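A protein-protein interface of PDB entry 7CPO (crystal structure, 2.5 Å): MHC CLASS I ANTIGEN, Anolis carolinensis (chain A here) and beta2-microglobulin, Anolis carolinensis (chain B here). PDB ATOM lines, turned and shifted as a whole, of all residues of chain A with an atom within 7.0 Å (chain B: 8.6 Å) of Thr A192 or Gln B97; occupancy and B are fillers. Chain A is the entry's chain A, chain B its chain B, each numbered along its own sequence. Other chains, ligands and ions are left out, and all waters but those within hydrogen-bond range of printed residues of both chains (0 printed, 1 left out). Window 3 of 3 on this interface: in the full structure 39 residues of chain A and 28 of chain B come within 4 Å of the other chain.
The side-chain hydroxyl (OG1) of Thr A192 is in hydrogen-bond range of the side-chain amide oxygen (OE1) of Gln B97 (2.9 Å). NZ of Lys A194 lies within salt-bridge range of OD2 of Asp B96 (3.2 Å). The backbone carbonyl oxygen (O) of Phe B11 lies within hydrogen-bond range of the guanidinium group (NH2) of Arg A206, at 3.3 Å.
O of Lys A190 lies within hydrogen-bond range of N of Arg A206. N of Thr A192 sits at hydrogen-bond distance from O of Ile A204, at 2.9 Å. The backbone carbonyl oxygen of Thr A202 sits at hydrogen-bond distance from the backbone NH of Lys A194 (3.1 Å).
His B13 touches Arg A206. NH1 of Arg A206 touches N of Pro B14, at 3.7 Å.
Of the printed residues of chain B, Thr A192 touches Gln B97. Printed residues of chain B within 4 Å of Lys A194: Asp B96. Of the printed residues of chain B, Arg A206 touches Phe B11 (3.3 Å), His B13 (3.8 Å) and Pro B14 (3.7 Å). Of the printed residues of chain A, Phe B11 touches Arg A206 (3.3 Å). Of the printed residues of chain A, His B13 touches Arg A206. Asp B73 touches none of the printed residues of chain A. Printed residues of chain A within 4 Å of Asp B96: Lys A194 (3.2 Å). Gln B97 touches just one residue of chain A: Thr A192 (2.9 Å).
Printed residues of chain B that touch a printed residue of chain A: Phe B11, His B13, Pro B14, Asp B96 and Gln B97. Among the printed residues, Asp or Glu carboxylates within 4 Å of a Lys or Arg side-chain nitrogen of the other chain: Lys A194 with Asp B96 (3.2 Å).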
ATOM      1  N   LYS A 190     -26.612   8.886   5.666  1.00  0.00           N
ATOM      2  CA  LYS A 190     -25.404   8.518   4.945  1.00  0.00           C
ATOM      3  C   LYS A 190     -25.415   9.209   3.588  1.00  0.00           C
ATOM      4  O   LYS A 190     -26.400   9.123   2.854  1.00  0.00           O
ATOM      5  CB  LYS A 190     -25.318   6.989   4.794  1.00  0.00           C
ATOM      6  CG  LYS A 190     -24.239   6.484   3.866  1.00  0.00           C
ATOM      7  CD  LYS A 190     -23.304   5.589   4.640  1.00  0.00           C
ATOM      8  CE  LYS A 190     -22.286   4.896   3.753  1.00  0.00           C
ATOM      9  NZ  LYS A 190     -22.939   3.892   2.901  1.00  0.00           N
ATOM     10  N   VAL A 191     -24.340   9.908   3.261  1.00  0.00           N
ATOM     11  CA  VAL A 191     -24.207  10.584   1.972  1.00  0.00           C
ATOM     12  C   VAL A 191     -23.275   9.769   1.093  1.00  0.00           C
ATOM     13  O   VAL A 191     -22.145   9.470   1.487  1.00  0.00           O
ATOM     14  CB  VAL A 191     -23.674  12.024   2.122  1.00  0.00           C
ATOM     15  CG1 VAL A 191     -23.661  12.708   0.763  1.00  0.00           C
ATOM     16  CG2 VAL A 191     -24.502  12.823   3.108  1.00  0.00           C
ATOM     17  N   THR A 192     -23.737   9.426  -0.101  1.00  0.00           N
ATOM     18  CA  THR A 192     -22.888   8.834  -1.114  1.00  0.00           C
ATOM     19  C   THR A 192     -22.809   9.744  -2.344  1.00  0.00           C
ATOM     20  O   THR A 192     -23.511  10.755  -2.459  1.00  0.00           O
ATOM     21  CB  THR A 192     -23.399   7.440  -1.489  1.00  0.00           C
ATOM     22  OG1 THR A 192     -24.773   7.536  -1.885  1.00  0.00           O
ATOM     23  CG2 THR A 192     -23.257   6.475  -0.305  1.00  0.00           C
ATOM     24  N   ARG A 193     -21.933   9.361  -3.275  1.00  0.00           N
ATOM     25  CA  ARG A 193     -21.590  10.144  -4.456  1.00  0.00           C
ATOM     26  C   ARG A 193     -21.504   9.181  -5.626  1.00  0.00           C
ATOM     27  O   ARG A 193     -20.811   8.168  -5.521  1.00  0.00           O
ATOM     28  CB  ARG A 193     -20.252  10.864  -4.236  1.00  0.00           C
ATOM     29  CG  ARG A 193     -19.699  11.587  -5.437  1.00  0.00           C
ATOM     30  CD  ARG A 193     -18.230  11.908  -5.205  1.00  0.00           C
ATOM     31  NE  ARG A 193     -17.408  10.713  -5.334  1.00  0.00           N
ATOM     32  CZ  ARG A 193     -16.982  10.225  -6.495  1.00  0.00           C
ATOM     33  NH1 ARG A 193     -17.287  10.843  -7.629  1.00  0.00           N
ATOM     34  NH2 ARG A 193     -16.243   9.125  -6.520  1.00  0.00           N
ATOM     35  N   LYS A 194     -22.176   9.483  -6.741  1.00  0.00           N
ATOM     36  CA  LYS A 194     -22.510   8.427  -7.696  1.00  0.00           C
ATOM     37  C   LYS A 194     -21.545   8.284  -8.875  1.00  0.00           C
ATOM     38  O   LYS A 194     -20.920   7.228  -9.020  1.00  0.00           O
ATOM     39  CB  LYS A 194     -23.946   8.601  -8.189  1.00  0.00           C
ATOM     40  CG  LYS A 194     -24.913   7.741  -7.387  1.00  0.00           C
ATOM     41  CD  LYS A 194     -25.010   6.316  -7.914  1.00  0.00           C
ATOM     42  CE  LYS A 194     -26.235   6.150  -8.800  1.00  0.00           C
ATOM     43  NZ  LYS A 194     -26.263   4.820  -9.461  1.00  0.00           N
ATOM     44  N   THR A 202     -24.040  13.131  -8.846  1.00  0.00           N
ATOM     45  CA  THR A 202     -25.260  13.107  -8.046  1.00  0.00           C
ATOM     46  C   THR A 202     -24.892  12.733  -6.613  1.00  0.00           C
ATOM     47  O   THR A 202     -24.308  11.666  -6.374  1.00  0.00           O
ATOM     48  CB  THR A 202     -26.291  12.125  -8.601  1.00  0.00           C
ATOM     49  OG1 THR A 202     -26.589  12.459  -9.958  1.00  0.00           O
ATOM     50  CG2 THR A 202     -27.589  12.204  -7.778  1.00  0.00           C
ATOM     51  N   LEU A 203     -25.214  13.615  -5.671  1.00  0.00           N
ATOM     52  CA  LEU A 203     -25.015  13.344  -4.253  1.00  0.00           C
ATOM     53  C   LEU A 203     -26.303  12.768  -3.667  1.00  0.00           C
ATOM     54  O   LEU A 203     -27.359  13.415  -3.720  1.00  0.00           O
ATOM     55  CB  LEU A 203     -24.598  14.618  -3.514  1.00  0.00           C
ATOM     56  CG  LEU A 203     -23.268  15.289  -3.909  1.00  0.00           C
ATOM     57  CD1 LEU A 203     -22.875  16.391  -2.913  1.00  0.00           C
ATOM     58  CD2 LEU A 203     -22.144  14.269  -4.060  1.00  0.00           C
ATOM     59  N   ILE A 204     -26.222  11.560  -3.110  1.00  0.00           N
ATOM     60  CA  ILE A 204     -27.391  10.870  -2.565  1.00  0.00           C
ATOM     61  C   ILE A 204     -27.349  10.907  -1.044  1.00  0.00           C
ATOM     62  O   ILE A 204     -26.339  10.547  -0.429  1.00  0.00           O
ATOM     63  CB  ILE A 204     -27.479   9.423  -3.065  1.00  0.00           C
ATOM     64  CG1 ILE A 204     -27.569   9.402  -4.587  1.00  0.00           C
ATOM     65  CG2 ILE A 204     -28.676   8.718  -2.437  1.00  0.00           C
ATOM     66  CD1 ILE A 204     -27.471   8.020  -5.155  1.00  0.00           C
ATOM     67  N   CYS A 205     -28.445  11.333  -0.435  1.00  0.00           N
ATOM     68  CA  CYS A 205     -28.582  11.313   1.018  1.00  0.00           C
ATOM     69  C   CYS A 205     -29.578  10.218   1.408  1.00  0.00           C
ATOM     70  O   CYS A 205     -30.782  10.359   1.167  1.00  0.00           O
ATOM     71  CB  CYS A 205     -29.026  12.680   1.524  1.00  0.00           C
ATOM     72  SG  CYS A 205     -29.113  12.726   3.289  1.00  0.00           S
ATOM     73  N   ARG A 206     -29.075   9.119   1.984  1.00  0.00           N
ATOM     74  CA  ARG A 206     -29.915   8.034   2.490  1.00  0.00           C
ATOM     75  C   ARG A 206     -30.199   8.279   3.965  1.00  0.00           C
ATOM     76  O   ARG A 206     -29.273   8.495   4.756  1.00  0.00           O
ATOM     77  CB  ARG A 206     -29.260   6.659   2.323  1.00  0.00           C
ATOM     78  CG  ARG A 206     -29.790   5.618   3.356  1.00  0.00           C
ATOM     79  CD  ARG A 206     -28.828   4.440   3.685  1.00  0.00           C
ATOM     80  NE  ARG A 206     -29.222   3.253   2.940  1.00  0.00           N
ATOM     81  CZ  ARG A 206     -29.995   2.278   3.405  1.00  0.00           C
ATOM     82  NH1 ARG A 206     -30.461   2.306   4.648  1.00  0.00           N
ATOM     83  NH2 ARG A 206     -30.297   1.266   2.615  1.00  0.00           N
ATOM     84  N   TRP A 219     -31.480  19.145   0.941  1.00  0.00           N
ATOM     85  CA  TRP A 219     -30.133  19.510   0.538  1.00  0.00           C
ATOM     86  C   TRP A 219     -29.943  21.024   0.660  1.00  0.00           C
ATOM     87  O   TRP A 219     -30.787  21.815   0.221  1.00  0.00           O
ATOM     88  CB  TRP A 219     -29.872  19.042  -0.888  1.00  0.00           C
ATOM     89  CG  TRP A 219     -29.408  17.646  -0.937  1.00  0.00           C
ATOM     90  CD1 TRP A 219     -30.135  16.546  -1.298  1.00  0.00           C
ATOM     91  CD2 TRP A 219     -28.100  17.177  -0.608  1.00  0.00           C
ATOM     92  NE1 TRP A 219     -29.357  15.425  -1.217  1.00  0.00           N
ATOM     93  CE2 TRP A 219     -28.102  15.781  -0.791  1.00  0.00           C
ATOM     94  CE3 TRP A 219     -26.923  17.806  -0.179  1.00  0.00           C
ATOM     95  CZ2 TRP A 219     -26.971  14.996  -0.559  1.00  0.00           C
ATOM     96  CZ3 TRP A 219     -25.802  17.031   0.053  1.00  0.00           C
ATOM     97  CH2 TRP A 219     -25.831  15.639  -0.141  1.00  0.00           C
ATOM     98  N   TYR A 244     -37.710   4.730   5.914  1.00  0.00           N
ATOM     99  CA  TYR A 244     -36.569   4.968   5.036  1.00  0.00           C
ATOM    100  C   TYR A 244     -36.957   5.904   3.895  1.00  0.00           C
ATOM    101  O   TYR A 244     -38.085   5.841   3.388  1.00  0.00           O
ATOM    102  CB  TYR A 244     -36.031   3.645   4.450  1.00  0.00           C
ATOM    103  CG  TYR A 244     -35.138   3.817   3.230  1.00  0.00           C
ATOM    104  CD1 TYR A 244     -35.678   3.808   1.947  1.00  0.00           C
ATOM    105  CD2 TYR A 244     -33.753   3.978   3.360  1.00  0.00           C
ATOM    106  CE1 TYR A 244     -34.887   3.970   0.829  1.00  0.00           C
ATOM    107  CE2 TYR A 244     -32.945   4.137   2.237  1.00  0.00           C
ATOM    108  CZ  TYR A 244     -33.524   4.131   0.977  1.00  0.00           C
ATOM    109  OH  TYR A 244     -32.758   4.275  -0.154  1.00  0.00           O
ATOM    110  N   ALA A 275     -22.238  16.035   4.843  1.00  0.00           N
ATOM    111  CA  ALA A 275     -21.594  16.198   3.544  1.00  0.00           C
ATOM    112  C   ALA A 275     -20.982  14.880   3.094  1.00  0.00           C
ATOM    113  O   ALA A 275     -20.894  13.912   3.854  1.00  0.00           O
ATOM    114  CB  ALA A 275     -20.510  17.278   3.599  1.00  0.00           C
ATOM    115  N   TRP A 276     -20.544  14.846   1.845  1.00  0.00           N
ATOM    116  CA  TRP A 276     -19.887  13.643   1.340  1.00  0.00           C
ATOM    117  C   TRP A 276     -18.550  13.386   2.057  1.00  0.00           C
ATOM    118  O   TRP A 276     -17.822  14.304   2.458  1.00  0.00           O
ATOM    119  CB  TRP A 276     -19.666  13.731  -0.164  1.00  0.00           C
ATOM    120  CG  TRP A 276     -18.944  12.552  -0.705  1.00  0.00           C
ATOM    121  CD1 TRP A 276     -19.441  11.290  -0.879  1.00  0.00           C
ATOM    122  CD2 TRP A 276     -17.580  12.507  -1.134  1.00  0.00           C
ATOM    123  NE1 TRP A 276     -18.473  10.464  -1.400  1.00  0.00           N
ATOM    124  CE2 TRP A 276     -17.320  11.187  -1.564  1.00  0.00           C
ATOM    125  CE3 TRP A 276     -16.550  13.455  -1.193  1.00  0.00           C
ATOM    126  CZ2 TRP A 276     -16.073  10.792  -2.053  1.00  0.00           C
ATOM    127  CZ3 TRP A 276     -15.313  13.061  -1.674  1.00  0.00           C
ATOM    128  CH2 TRP A 276     -15.088  11.743  -2.101  1.00  0.00           C
ATOM    129  OXT TRP A 276     -18.174  12.225   2.275  1.00  0.00           O
ATOM    130  N   PHE B  11     -32.618  -1.722   1.717  1.00  0.00           N
ATOM    131  CA  PHE B  11     -32.229  -2.474   2.897  1.00  0.00           C
ATOM    132  C   PHE B  11     -32.570  -1.681   4.147  1.00  0.00           C
ATOM    133  O   PHE B  11     -32.645  -0.451   4.119  1.00  0.00           O
ATOM    134  CB  PHE B  11     -30.723  -2.747   2.918  1.00  0.00           C
ATOM    135  CG  PHE B  11     -30.261  -3.809   1.968  1.00  0.00           C
ATOM    136  CD1 PHE B  11     -30.976  -4.975   1.802  1.00  0.00           C
ATOM    137  CD2 PHE B  11     -29.075  -3.644   1.271  1.00  0.00           C
ATOM    138  CE1 PHE B  11     -30.530  -5.953   0.938  1.00  0.00           C
ATOM    139  CE2 PHE B  11     -28.628  -4.609   0.407  1.00  0.00           C
ATOM    140  CZ  PHE B  11     -29.354  -5.767   0.235  1.00  0.00           C
ATOM    141  N   HIS B  13     -30.492  -1.527   6.765  1.00  0.00           N
ATOM    142  CA  HIS B  13     -29.214  -0.848   6.930  1.00  0.00           C
ATOM    143  C   HIS B  13     -28.448  -0.832   5.608  1.00  0.00           C
ATOM    144  O   HIS B  13     -28.661  -1.699   4.753  1.00  0.00           O
ATOM    145  CB  HIS B  13     -28.337  -1.523   7.994  1.00  0.00           C
ATOM    146  CG  HIS B  13     -29.038  -1.791   9.287  1.00  0.00           C
ATOM    147  ND1 HIS B  13     -29.188  -0.832  10.266  1.00  0.00           N
ATOM    148  CD2 HIS B  13     -29.602  -2.922   9.774  1.00  0.00           C
ATOM    149  CE1 HIS B  13     -29.826  -1.358  11.297  1.00  0.00           C
ATOM    150  NE2 HIS B  13     -30.088  -2.624  11.023  1.00  0.00           N
ATOM    151  N   PRO B  14     -27.556   0.138   5.407  1.00  0.00           N
ATOM    152  CA  PRO B  14     -26.617   0.047   4.277  1.00  0.00           C
ATOM    153  C   PRO B  14     -25.827  -1.257   4.351  1.00  0.00           C
ATOM    154  O   PRO B  14     -25.361  -1.657   5.421  1.00  0.00           O
ATOM    155  CB  PRO B  14     -25.713   1.274   4.461  1.00  0.00           C
ATOM    156  CG  PRO B  14     -25.866   1.656   5.924  1.00  0.00           C
ATOM    157  CD  PRO B  14     -27.279   1.289   6.287  1.00  0.00           C
ATOM    158  N   ALA B  15     -25.686  -1.920   3.199  1.00  0.00           N
ATOM    159  CA  ALA B  15     -25.189  -3.293   3.155  1.00  0.00           C
ATOM    160  C   ALA B  15     -23.777  -3.428   3.740  1.00  0.00           C
ATOM    161  O   ALA B  15     -22.988  -2.479   3.776  1.00  0.00           O
ATOM    162  CB  ALA B  15     -25.210  -3.815   1.716  1.00  0.00           C
ATOM    163  N   GLU B  16     -23.478  -4.633   4.223  1.00  0.00           N
ATOM    164  CA  GLU B  16     -22.151  -5.030   4.677  1.00  0.00           C
ATOM    165  C   GLU B  16     -22.022  -6.521   4.407  1.00  0.00           C
ATOM    166  O   GLU B  16     -22.953  -7.281   4.697  1.00  0.00           O
ATOM    167  CB  GLU B  16     -21.937  -4.751   6.170  1.00  0.00           C
ATOM    168  CG  GLU B  16     -21.858  -3.287   6.543  1.00  0.00           C
ATOM    169  CD  GLU B  16     -20.780  -3.001   7.568  1.00  0.00           C
ATOM    170  OE1 GLU B  16     -21.120  -2.816   8.758  1.00  0.00           O
ATOM    171  OE2 GLU B  16     -19.592  -2.956   7.179  1.00  0.00           O
ATOM    172  N   PRO B  72     -25.910  -9.813   2.936  1.00  0.00           N
ATOM    173  CA  PRO B  72     -25.224  -9.313   1.740  1.00  0.00           C
ATOM    174  C   PRO B  72     -23.795  -9.843   1.587  1.00  0.00           C
ATOM    175  O   PRO B  72     -23.141 -10.256   2.550  1.00  0.00           O
ATOM    176  CB  PRO B  72     -25.235  -7.790   1.933  1.00  0.00           C
ATOM    177  CG  PRO B  72     -26.414  -7.528   2.850  1.00  0.00           C
ATOM    178  CD  PRO B  72     -26.491  -8.724   3.755  1.00  0.00           C
ATOM    179  N   ASP B  73     -23.340  -9.852   0.333  1.00  0.00           N
ATOM    180  CA  ASP B  73     -21.934  -9.938  -0.045  1.00  0.00           C
ATOM    181  C   ASP B  73     -21.785  -9.214  -1.380  1.00  0.00           C
ATOM    182  O   ASP B  73     -22.774  -8.895  -2.047  1.00  0.00           O
ATOM    183  CB  ASP B  73     -21.450 -11.389  -0.131  1.00  0.00           C
ATOM    184  CG  ASP B  73     -22.405 -12.272  -0.901  1.00  0.00           C
ATOM    185  OD1 ASP B  73     -22.732 -13.360  -0.390  1.00  0.00           O
ATOM    186  OD2 ASP B  73     -22.831 -11.883  -2.011  1.00  0.00           O
ATOM    187  N   GLY B  74     -20.544  -8.953  -1.773  1.00  0.00           N
ATOM    188  CA  GLY B  74     -20.290  -8.199  -2.990  1.00  0.00           C
ATOM    189  C   GLY B  74     -20.855  -8.835  -4.245  1.00  0.00           C
ATOM    190  O   GLY B  74     -21.353  -9.964  -4.217  1.00  0.00           O
ATOM    191  N   ALA B  76     -23.425 -10.204  -5.235  1.00  0.00           N
ATOM    192  CA  ALA B  76     -24.785 -10.734  -5.324  1.00  0.00           C
ATOM    193  C   ALA B  76     -25.810  -9.599  -5.397  1.00  0.00           C
ATOM    194  O   ALA B  76     -25.757  -8.666  -4.597  1.00  0.00           O
ATOM    195  CB  ALA B  76     -25.072 -11.632  -4.144  1.00  0.00           C
ATOM    196  N   GLU B  77     -26.742  -9.688  -6.349  1.00  0.00           N
ATOM    197  CA  GLU B  77     -27.620  -8.580  -6.726  1.00  0.00           C
ATOM    198  C   GLU B  77     -29.054  -8.799  -6.248  1.00  0.00           C
ATOM    199  O   GLU B  77     -29.593  -9.905  -6.353  1.00  0.00           O
ATOM    200  CB  GLU B  77     -27.629  -8.388  -8.248  1.00  0.00           C
ATOM    201  CG  GLU B  77     -26.554  -7.440  -8.768  1.00  0.00           C
ATOM    202  CD  GLU B  77     -26.015  -7.859 -10.120  1.00  0.00           C
ATOM    203  OE1 GLU B  77     -24.825  -7.578 -10.399  1.00  0.00           O
ATOM    204  OE2 GLU B  77     -26.786  -8.469 -10.898  1.00  0.00           O
ATOM    205  N   PHE B  78     -29.686  -7.728  -5.769  1.00  0.00           N
ATOM    206  CA  PHE B  78     -31.040  -7.773  -5.232  1.00  0.00           C
ATOM    207  C   PHE B  78     -31.976  -6.896  -6.049  1.00  0.00           C
ATOM    208  O   PHE B  78     -31.627  -5.767  -6.416  1.00  0.00           O
ATOM    209  CB  PHE B  78     -31.051  -7.320  -3.780  1.00  0.00           C
ATOM    210  CG  PHE B  78     -30.192  -8.157  -2.892  1.00  0.00           C
ATOM    211  CD1 PHE B  78     -30.669  -9.345  -2.373  1.00  0.00           C
ATOM    212  CD2 PHE B  78     -28.893  -7.769  -2.597  1.00  0.00           C
ATOM    213  CE1 PHE B  78     -29.882 -10.122  -1.563  1.00  0.00           C
ATOM    214  CE2 PHE B  78     -28.100  -8.536  -1.779  1.00  0.00           C
ATOM    215  CZ  PHE B  78     -28.595  -9.717  -1.259  1.00  0.00           C
ATOM    216  N   LYS B  94     -34.115  -2.661  -9.540  1.00  0.00           N
ATOM    217  CA  LYS B  94     -32.838  -3.114  -9.014  1.00  0.00           C
ATOM    218  C   LYS B  94     -32.424  -2.226  -7.850  1.00  0.00           C
ATOM    219  O   LYS B  94     -32.666  -1.016  -7.844  1.00  0.00           O
ATOM    220  CB  LYS B  94     -31.745  -3.097 -10.099  1.00  0.00           C
ATOM    221  CG  LYS B  94     -32.134  -3.669 -11.484  1.00  0.00           C
ATOM    222  CD  LYS B  94     -31.240  -4.843 -11.932  1.00  0.00           C
ATOM    223  CE  LYS B  94     -31.776  -5.548 -13.202  1.00  0.00           C
ATOM    224  NZ  LYS B  94     -32.203  -6.983 -12.957  1.00  0.00           N
ATOM    225  N   LEU B  95     -31.790  -2.833  -6.862  1.00  0.00           N
ATOM    226  CA  LEU B  95     -31.278  -2.099  -5.718  1.00  0.00           C
ATOM    227  C   LEU B  95     -29.797  -1.829  -5.937  1.00  0.00           C
ATOM    228  O   LEU B  95     -29.036  -2.754  -6.244  1.00  0.00           O
ATOM    229  CB  LEU B  95     -31.492  -2.902  -4.436  1.00  0.00           C
ATOM    230  CG  LEU B  95     -30.680  -2.486  -3.216  1.00  0.00           C
ATOM    231  CD1 LEU B  95     -31.304  -1.261  -2.591  1.00  0.00           C
ATOM    232  CD2 LEU B  95     -30.639  -3.625  -2.227  1.00  0.00           C
ATOM    233  N   ASP B  96     -29.374  -0.578  -5.793  1.00  0.00           N
ATOM    234  CA  ASP B  96     -27.950  -0.310  -5.942  1.00  0.00           C
ATOM    235  C   ASP B  96     -27.366   0.203  -4.634  1.00  0.00           C
ATOM    236  O   ASP B  96     -28.086   0.746  -3.788  1.00  0.00           O
ATOM    237  CB  ASP B  96     -27.651   0.654  -7.114  1.00  0.00           C
ATOM    238  CG  ASP B  96     -28.048   2.082  -6.829  1.00  0.00           C
ATOM    239  OD1 ASP B  96     -29.196   2.303  -6.391  1.00  0.00           O
ATOM    240  OD2 ASP B  96     -27.217   2.982  -7.071  1.00  0.00           O
ATOM    241  N   GLN B  97     -26.055  -0.031  -4.489  1.00  0.00           N
ATOM    242  CA  GLN B  97     -25.170   0.316  -3.357  1.00  0.00           C
ATOM    243  C   GLN B  97     -24.991  -0.883  -2.401  1.00  0.00           C
ATOM    244  O   GLN B  97     -23.988  -0.956  -1.680  1.00  0.00           O
ATOM    245  CB  GLN B  97     -25.661   1.564  -2.591  1.00  0.00           C
ATOM    246  CG  GLN B  97     -25.855   2.817  -3.473  1.00  0.00           C
ATOM    247  CD  GLN B  97     -25.828   4.111  -2.681  1.00  0.00           C
ATOM    248  OE1 GLN B  97     -24.759   4.637  -2.390  1.00  0.00           O
ATOM    249  NE2 GLN B  97     -27.012   4.632  -2.330  1.00  0.00           N
